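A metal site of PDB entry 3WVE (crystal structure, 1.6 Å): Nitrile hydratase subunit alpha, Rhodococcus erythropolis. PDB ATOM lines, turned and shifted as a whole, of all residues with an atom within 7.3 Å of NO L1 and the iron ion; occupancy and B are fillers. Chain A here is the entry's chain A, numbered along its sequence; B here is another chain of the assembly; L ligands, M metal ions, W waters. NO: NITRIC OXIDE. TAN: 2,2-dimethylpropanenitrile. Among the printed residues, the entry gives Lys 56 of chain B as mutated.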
ATOM      1  N   GLN A  91     -26.947  15.984 -19.308  1.00  0.00           N
ATOM      2  CA  GLN A  91     -25.838  15.289 -18.686  1.00  0.00           C
ATOM      3  C   GLN A  91     -26.001  13.780 -18.812  1.00  0.00           C
ATOM      4  O   GLN A  91     -25.555  12.996 -18.006  1.00  0.00           O
ATOM      5  CB  GLN A  91     -25.553  15.688 -17.238  1.00  0.00           C
ATOM      6  CG  GLN A  91     -25.196  17.179 -17.128  1.00  0.00           C
ATOM      7  CD  GLN A  91     -23.978  17.455 -17.825  1.00  0.00           C
ATOM      8  OE1 GLN A  91     -22.956  16.839 -17.563  1.00  0.00           O
ATOM      9  NE2 GLN A  91     -24.046  18.367 -18.725  1.00  0.00           N
ATOM     10  N   VAL A 109     -15.825   7.836 -11.887  1.00  0.00           N
ATOM     11  CA  VAL A 109     -15.573   9.119 -11.160  1.00  0.00           C
ATOM     12  C   VAL A 109     -15.597  10.273 -12.178  1.00  0.00           C
ATOM     13  O   VAL A 109     -15.435  10.052 -13.413  1.00  0.00           O
ATOM     14  CB  VAL A 109     -14.201   9.017 -10.451  1.00  0.00           C
ATOM     15  CG1 VAL A 109     -13.061   8.883 -11.421  1.00  0.00           C
ATOM     16  CG2 VAL A 109     -13.925  10.198  -9.533  1.00  0.00           C
ATOM     17  N   CYS A 110     -15.655  11.504 -11.641  1.00  0.00           N
ATOM     18  CA  CYS A 110     -15.297  12.684 -12.344  1.00  0.00           C
ATOM     19  C   CYS A 110     -14.215  13.388 -11.529  1.00  0.00           C
ATOM     20  O   CYS A 110     -14.535  14.093 -10.527  1.00  0.00           O
ATOM     21  CB  CYS A 110     -16.478  13.618 -12.572  1.00  0.00           C
ATOM     22  SG  CYS A 110     -15.991  15.149 -13.427  1.00  0.00           S
ATOM     23  N   SER A 111     -12.943  13.142 -11.838  1.00  0.00           N
ATOM     24  CA  SER A 111     -11.895  13.671 -10.995  1.00  0.00           C
ATOM     25  C   SER A 111     -11.872  15.204 -11.027  1.00  0.00           C
ATOM     26  O   SER A 111     -11.421  15.836 -10.085  1.00  0.00           O
ATOM     27  CB  SER A 111     -10.540  13.161 -11.343  1.00  0.00           C
ATOM     28  OG  SER A 111     -10.075  13.567 -12.609  1.00  0.00           O
ATOM     29  N   LEU A 112     -12.310  15.803 -12.139  1.00  0.00           N
ATOM     30  CA  LEU A 112     -12.237  17.225 -12.343  1.00  0.00           C
ATOM     31  C   LEU A 112     -13.403  18.015 -11.769  1.00  0.00           C
ATOM     32  O   LEU A 112     -13.259  19.234 -11.630  1.00  0.00           O
ATOM     33  CB  LEU A 112     -12.120  17.500 -13.834  1.00  0.00           C
ATOM     34  CG  LEU A 112     -10.834  17.010 -14.493  1.00  0.00           C
ATOM     35  CD1 LEU A 112     -10.879  17.035 -16.002  1.00  0.00           C
ATOM     36  CD2 LEU A 112      -9.553  17.706 -14.012  1.00  0.00           C
ATOM     37  N   CSD A 113     -14.504  17.347 -11.407  1.00  0.00           N
ATOM     38  CA  CSD A 113     -15.709  18.035 -10.922  1.00  0.00           C
ATOM     39  CB  CSD A 113     -16.271  18.954 -12.004  1.00  0.00           C
ATOM     40  SG  CSD A 113     -16.569  18.333 -13.601  1.00  0.00           S
ATOM     41  C   CSD A 113     -16.728  17.044 -10.426  1.00  0.00           C
ATOM     42  O   CSD A 113     -16.703  16.713  -9.211  1.00  0.00           O
ATOM     43  OD1 CSD A 113     -17.257  19.443 -14.340  1.00  0.00           O
ATOM     44  OD2 CSD A 113     -15.217  18.106 -14.167  1.00  0.00           O
ATOM     45  N   SER A 114     -17.694  16.583 -11.224  1.00  0.00           N
ATOM     46  CA  SER A 114     -18.769  15.716 -10.680  1.00  0.00           C
ATOM     47  C   SER A 114     -19.527  14.957 -11.724  1.00  0.00           C
ATOM     48  O   SER A 114     -20.497  14.264 -11.404  1.00  0.00           O
ATOM     49  CB  SER A 114     -19.725  16.571  -9.897  1.00  0.00           C
ATOM     50  OG  SER A 114     -20.507  17.459 -10.775  1.00  0.00           O
ATOM     51  N   CSO A 115     -19.064  15.059 -12.941  1.00  0.00           N
ATOM     52  CA  CSO A 115     -19.723  14.510 -14.112  1.00  0.00           C
ATOM     53  CB  CSO A 115     -18.800  14.561 -15.338  1.00  0.00           C
ATOM     54  SG  CSO A 115     -17.975  16.134 -15.465  1.00  0.00           S
ATOM     55  C   CSO A 115     -20.300  13.098 -13.824  1.00  0.00           C
ATOM     56  O   CSO A 115     -19.554  12.162 -13.439  1.00  0.00           O
ATOM     57  N   THR A 116     -21.576  12.936 -14.134  1.00  0.00           N
ATOM     58  CA  THR A 116     -22.428  11.808 -13.792  1.00  0.00           C
ATOM     59  C   THR A 116     -23.495  11.748 -14.841  1.00  0.00           C
ATOM     60  O   THR A 116     -24.032  12.781 -15.259  1.00  0.00           O
ATOM     61  CB  THR A 116     -23.067  12.053 -12.391  1.00  0.00           C
ATOM     62  OG1 THR A 116     -22.047  12.054 -11.421  1.00  0.00           O
ATOM     63  CG2 THR A 116     -24.169  11.114 -12.042  1.00  0.00           C
ATOM     64  N   TRP A 118     -26.705  11.932 -15.037  1.00  0.00           N
ATOM     65  CA  TRP A 118     -27.813  12.346 -14.203  1.00  0.00           C
ATOM     66  C   TRP A 118     -29.171  11.595 -14.430  1.00  0.00           C
ATOM     67  O   TRP A 118     -29.798  11.243 -13.453  1.00  0.00           O
ATOM     68  CB  TRP A 118     -28.104  13.860 -14.395  1.00  0.00           C
ATOM     69  CG  TRP A 118     -27.089  14.784 -13.874  1.00  0.00           C
ATOM     70  CD1 TRP A 118     -25.995  14.518 -13.086  1.00  0.00           C
ATOM     71  CD2 TRP A 118     -27.119  16.197 -14.063  1.00  0.00           C
ATOM     72  NE1 TRP A 118     -25.355  15.704 -12.776  1.00  0.00           N
ATOM     73  CE2 TRP A 118     -26.036  16.741 -13.341  1.00  0.00           C
ATOM     74  CE3 TRP A 118     -27.989  17.045 -14.758  1.00  0.00           C
ATOM     75  CZ2 TRP A 118     -25.753  18.112 -13.335  1.00  0.00           C
ATOM     76  CZ3 TRP A 118     -27.672  18.432 -14.751  1.00  0.00           C
ATOM     77  CH2 TRP A 118     -26.588  18.933 -14.002  1.00  0.00           C
ATOM     78  N   PRO A 124     -25.287  13.388  -8.598  1.00  0.00           N
ATOM     79  CA  PRO A 124     -24.300  12.706  -7.797  1.00  0.00           C
ATOM     80  C   PRO A 124     -24.474  12.986  -6.316  1.00  0.00           C
ATOM     81  O   PRO A 124     -24.879  14.082  -5.961  1.00  0.00           O
ATOM     82  CB  PRO A 124     -22.954  13.257  -8.282  1.00  0.00           C
ATOM     83  CG  PRO A 124     -23.333  14.572  -8.938  1.00  0.00           C
ATOM     84  CD  PRO A 124     -24.675  14.282  -9.590  1.00  0.00           C
ATOM     85  N   TYR A 128     -19.415  11.462  -3.850  1.00  0.00           N
ATOM     86  CA  TYR A 128     -18.862  11.202  -5.166  1.00  0.00           C
ATOM     87  C   TYR A 128     -18.162  12.473  -5.624  1.00  0.00           C
ATOM     88  O   TYR A 128     -17.195  12.443  -6.341  1.00  0.00           O
ATOM     89  CB  TYR A 128     -19.949  10.844  -6.129  1.00  0.00           C
ATOM     90  CG  TYR A 128     -19.616  10.651  -7.548  1.00  0.00           C
ATOM     91  CD1 TYR A 128     -19.636  11.742  -8.414  1.00  0.00           C
ATOM     92  CD2 TYR A 128     -19.328   9.422  -8.072  1.00  0.00           C
ATOM     93  CE1 TYR A 128     -19.351  11.615  -9.757  1.00  0.00           C
ATOM     94  CE2 TYR A 128     -19.011   9.275  -9.366  1.00  0.00           C
ATOM     95  CZ  TYR A 128     -19.044  10.345 -10.256  1.00  0.00           C
ATOM     96  OH  TYR A 128     -18.866  10.175 -11.594  1.00  0.00           O
ATOM     97  N   ARG A 134     -12.536  12.070  -5.535  1.00  0.00           N
ATOM     98  CA  ARG A 134     -11.965  12.601  -6.760  1.00  0.00           C
ATOM     99  C   ARG A 134     -10.433  12.432  -6.833  1.00  0.00           C
ATOM    100  O   ARG A 134      -9.866  12.218  -7.891  1.00  0.00           O
ATOM    101  CB  ARG A 134     -12.329  14.122  -6.885  1.00  0.00           C
ATOM    102  CG  ARG A 134     -13.754  14.330  -7.228  1.00  0.00           C
ATOM    103  CD  ARG A 134     -14.186  15.791  -7.213  1.00  0.00           C
ATOM    104  NE  ARG A 134     -13.298  16.585  -8.055  1.00  0.00           N
ATOM    105  CZ  ARG A 134     -13.108  17.870  -7.924  1.00  0.00           C
ATOM    106  NH1 ARG A 134     -13.827  18.592  -7.081  1.00  0.00           N
ATOM    107  NH2 ARG A 134     -12.179  18.468  -8.643  1.00  0.00           N
ATOM    108  N   THR A 163     -14.683  10.576 -16.020  1.00  0.00           N
ATOM    109  CA  THR A 163     -15.685  11.204 -16.840  1.00  0.00           C
ATOM    110  C   THR A 163     -15.278  12.629 -17.245  1.00  0.00           C
ATOM    111  O   THR A 163     -15.837  13.603 -16.775  1.00  0.00           O
ATOM    112  CB  THR A 163     -17.062  11.149 -16.131  1.00  0.00           C
ATOM    113  OG1 THR A 163     -17.355   9.820 -15.689  1.00  0.00           O
ATOM    114  CG2 THR A 163     -18.175  11.593 -17.070  1.00  0.00           C
ATOM    115  N   THR A 164     -14.348  12.710 -18.196  1.00  0.00           N
ATOM    116  CA  THR A 164     -13.657  13.941 -18.539  1.00  0.00           C
ATOM    117  C   THR A 164     -14.239  14.708 -19.735  1.00  0.00           C
ATOM    118  O   THR A 164     -13.818  15.818 -19.991  1.00  0.00           O
ATOM    119  CB  THR A 164     -12.165  13.659 -18.764  1.00  0.00           C
ATOM    120  OG1 THR A 164     -12.046  12.495 -19.656  1.00  0.00           O
ATOM    121  CG2 THR A 164     -11.474  13.316 -17.475  1.00  0.00           C
ATOM    122  N   ARG A 168     -21.170   9.683 -20.727  1.00  0.00           N
ATOM    123  CA  ARG A 168     -21.696   9.476 -19.394  1.00  0.00           C
ATOM    124  C   ARG A 168     -21.889   8.016 -19.199  1.00  0.00           C
ATOM    125  O   ARG A 168     -22.431   7.293 -20.095  1.00  0.00           O
ATOM    126  CB  ARG A 168     -22.969  10.283 -19.197  1.00  0.00           C
ATOM    127  CG  ARG A 168     -22.746  11.746 -19.304  1.00  0.00           C
ATOM    128  CD  ARG A 168     -22.108  12.349 -18.044  1.00  0.00           C
ATOM    129  NE  ARG A 168     -21.808  13.776 -18.169  1.00  0.00           N
ATOM    130  CZ  ARG A 168     -20.765  14.265 -18.765  1.00  0.00           C
ATOM    131  NH1 ARG A 168     -19.892  13.486 -19.296  1.00  0.00           N
ATOM    132  NH2 ARG A 168     -20.594  15.566 -18.893  1.00  0.00           N
ATOM    133  N   TYR B  37     -27.737  24.736 -10.454  1.00  0.00           N
ATOM    134  CA  TYR B  37     -27.970  24.039 -11.681  1.00  0.00           C
ATOM    135  C   TYR B  37     -29.120  24.623 -12.498  1.00  0.00           C
ATOM    136  O   TYR B  37     -29.018  24.707 -13.717  1.00  0.00           O
ATOM    137  CB  TYR B  37     -28.221  22.533 -11.471  1.00  0.00           C
ATOM    138  CG  TYR B  37     -27.094  21.669 -10.994  1.00  0.00           C
ATOM    139  CD1 TYR B  37     -25.760  22.042 -10.965  1.00  0.00           C
ATOM    140  CD2 TYR B  37     -27.377  20.365 -10.629  1.00  0.00           C
ATOM    141  CE1 TYR B  37     -24.758  21.124 -10.586  1.00  0.00           C
ATOM    142  CE2 TYR B  37     -26.394  19.461 -10.286  1.00  0.00           C
ATOM    143  CZ  TYR B  37     -25.088  19.840 -10.253  1.00  0.00           C
ATOM    144  OH  TYR B  37     -24.113  18.911  -9.942  1.00  0.00           O
ATOM    145  N   VAL B  52     -21.920  25.264 -21.085  1.00  0.00           N
ATOM    146  CA  VAL B  52     -21.630  24.399 -19.860  1.00  0.00           C
ATOM    147  C   VAL B  52     -20.124  24.454 -19.607  1.00  0.00           C
ATOM    148  O   VAL B  52     -19.650  24.511 -18.446  1.00  0.00           O
ATOM    149  CB  VAL B  52     -22.152  22.966 -20.029  1.00  0.00           C
ATOM    150  CG1 VAL B  52     -21.762  22.081 -18.857  1.00  0.00           C
ATOM    151  CG2 VAL B  52     -23.675  23.010 -20.134  1.00  0.00           C
ATOM    152  N   LYS B  56     -17.815  25.045 -16.128  1.00  0.00           N
ATOM    153  CA  LYS B  56     -16.707  24.243 -15.578  1.00  0.00           C
ATOM    154  C   LYS B  56     -15.503  25.151 -15.353  1.00  0.00           C
ATOM    155  O   LYS B  56     -14.849  25.075 -14.282  1.00  0.00           O
ATOM    156  CB  LYS B  56     -16.391  23.064 -16.457  1.00  0.00           C
ATOM    157  CG  LYS B  56     -17.539  22.093 -16.659  1.00  0.00           C
ATOM    158  CD  LYS B  56     -17.168  20.863 -17.467  1.00  0.00           C
ATOM    159  CE  LYS B  56     -18.406  19.967 -17.560  1.00  0.00           C
ATOM    160  NZ  LYS B  56     -18.121  18.617 -18.052  1.00  0.00           N
ATOM    161  N   TYR B  72     -19.462  21.910  -2.632  1.00  0.00           N
ATOM    162  CA  TYR B  72     -19.800  21.727  -4.031  1.00  0.00           C
ATOM    163  C   TYR B  72     -20.851  22.699  -4.562  1.00  0.00           C
ATOM    164  O   TYR B  72     -20.578  23.425  -5.488  1.00  0.00           O
ATOM    165  CB  TYR B  72     -20.231  20.261  -4.279  1.00  0.00           C
ATOM    166  CG  TYR B  72     -20.637  20.048  -5.723  1.00  0.00           C
ATOM    167  CD1 TYR B  72     -19.719  19.682  -6.669  1.00  0.00           C
ATOM    168  CD2 TYR B  72     -21.943  20.194  -6.094  1.00  0.00           C
ATOM    169  CE1 TYR B  72     -20.062  19.524  -7.963  1.00  0.00           C
ATOM    170  CE2 TYR B  72     -22.336  20.080  -7.423  1.00  0.00           C
ATOM    171  CZ  TYR B  72     -21.366  19.705  -8.382  1.00  0.00           C
ATOM    172  OH  TYR B  72     -21.632  19.573  -9.732  1.00  0.00           O
ATOM    173  N   TYR B  76     -20.822  26.382  -7.472  1.00  0.00           N
ATOM    174  CA  TYR B  76     -21.634  26.665  -8.701  1.00  0.00           C
ATOM    175  C   TYR B  76     -22.474  27.931  -8.544  1.00  0.00           C
ATOM    176  O   TYR B  76     -22.680  28.610  -9.538  1.00  0.00           O
ATOM    177  CB  TYR B  76     -22.449  25.416  -9.167  1.00  0.00           C
ATOM    178  CG  TYR B  76     -21.479  24.331  -9.618  1.00  0.00           C
ATOM    179  CD1 TYR B  76     -21.037  24.217 -10.925  1.00  0.00           C
ATOM    180  CD2 TYR B  76     -20.862  23.544  -8.647  1.00  0.00           C
ATOM    181  CE1 TYR B  76     -20.076  23.308 -11.284  1.00  0.00           C
ATOM    182  CE2 TYR B  76     -19.884  22.636  -9.008  1.00  0.00           C
ATOM    183  CZ  TYR B  76     -19.457  22.540 -10.323  1.00  0.00           C
ATOM    184  OH  TYR B  76     -18.507  21.622 -10.643  1.00  0.00           O
ATOM    185  N   ARG B 141      -9.910  19.731 -20.811  1.00  0.00           N
ATOM    186  CA  ARG B 141     -10.524  18.529 -20.237  1.00  0.00           C
ATOM    187  C   ARG B 141      -9.533  17.331 -20.273  1.00  0.00           C
ATOM    188  O   ARG B 141      -9.835  16.209 -20.598  1.00  0.00           O
ATOM    189  CB  ARG B 141     -11.848  18.218 -20.946  1.00  0.00           C
ATOM    190  CG  ARG B 141     -12.916  19.236 -20.689  1.00  0.00           C
ATOM    191  CD  ARG B 141     -13.184  19.465 -19.204  1.00  0.00           C
ATOM    192  NE  ARG B 141     -13.704  18.292 -18.567  1.00  0.00           N
ATOM    193  CZ  ARG B 141     -14.132  18.249 -17.305  1.00  0.00           C
ATOM    194  NH1 ARG B 141     -13.817  19.266 -16.505  1.00  0.00           N
ATOM    195  NH2 ARG B 141     -14.836  17.242 -16.875  1.00  0.00           N
HETATM  196  N    NO L   1     -19.339  17.865 -13.325  1.00  0.00           N
HETATM  197  O    NO L   1     -20.383  17.700 -14.032  1.00  0.00           O
HETATM  198  C   TAN L   2     -22.917  22.498 -13.895  1.00  0.00           C
HETATM  199  N   TAN L   2     -23.501  23.469 -13.565  1.00  0.00           N
HETATM  200  C1  TAN L   2     -22.192  20.396 -13.111  1.00  0.00           C
HETATM  201  C2  TAN L   2     -22.197  21.325 -14.266  1.00  0.00           C
HETATM  202  C3  TAN L   2     -20.951  21.513 -15.027  1.00  0.00           C
HETATM  203  C4  TAN L   2     -23.076  20.698 -15.341  1.00  0.00           C
HETATM  204 FE    FE M   1     -17.823  16.578 -13.272  1.00  0.00          FE
HETATM  205  O   HOH W   1     -22.896  15.590 -14.889  1.00  0.00           O
HETATM  206  O   HOH W   2     -22.664  16.183 -11.985  1.00  0.00           O
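Water W2 lies within hydrogen-bond range of the side-chain hydroxyl of Ser 114, the indole nitrogen of Trp 118 and an oxygen (O) of NO L1.
The iron ion is bound by N of CSO 115. N of NO L1 binds the iron ion. The iron ion is bound by N of Ser 114 (2.1 Å). The iron ion is bound by SG of CSD 113, 2.2 Å away. SG of CSO 115 is bound to the iron ion (2.2 Å). SG of Cys 110 binds the iron ion (2.3 Å). The iron ion has six donor atoms within binding distance.
NZ of Lys 56 of chain B lies within salt-bridge range of OD1 of CSD 113, 3.9 Å away. The side-chain sulfur (SG) of Cys 110 lies close to the backbone carbonyl oxygen (O) of Thr 163. SG of CSO 115 sits close to NZ of Lys 56 of chain B, 3.6 Å away. O of CSO 115 lies within hydrogen-bond range of OH of Tyr 128 (2.8 Å). NH2 of Arg 141 of chain B lies close to SG of CSO 115. The backbone NH of Cys 110 sits at hydrogen-bond distance from the side-chain hydroxyl of Tyr 128 (3.5 Å). OD2 of CSD 113 is in salt-bridge range of NH2 of Arg 141 of chain B, at 2.9 Å. The side-chain hydroxyl (OG) of Ser 114 lies within hydrogen-bond range of the side-chain hydroxyl (OH) of Tyr 72 of chain B (2.6 Å).
Along chain A the residues within 4 Å of the iron ion span positions 110 to 115.
OG of Ser 114 is in hydrogen-bond range of O of NO L1 (3.3 Å).
Of the 22 residues printed, 3 come within 4 Å of NO L1.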
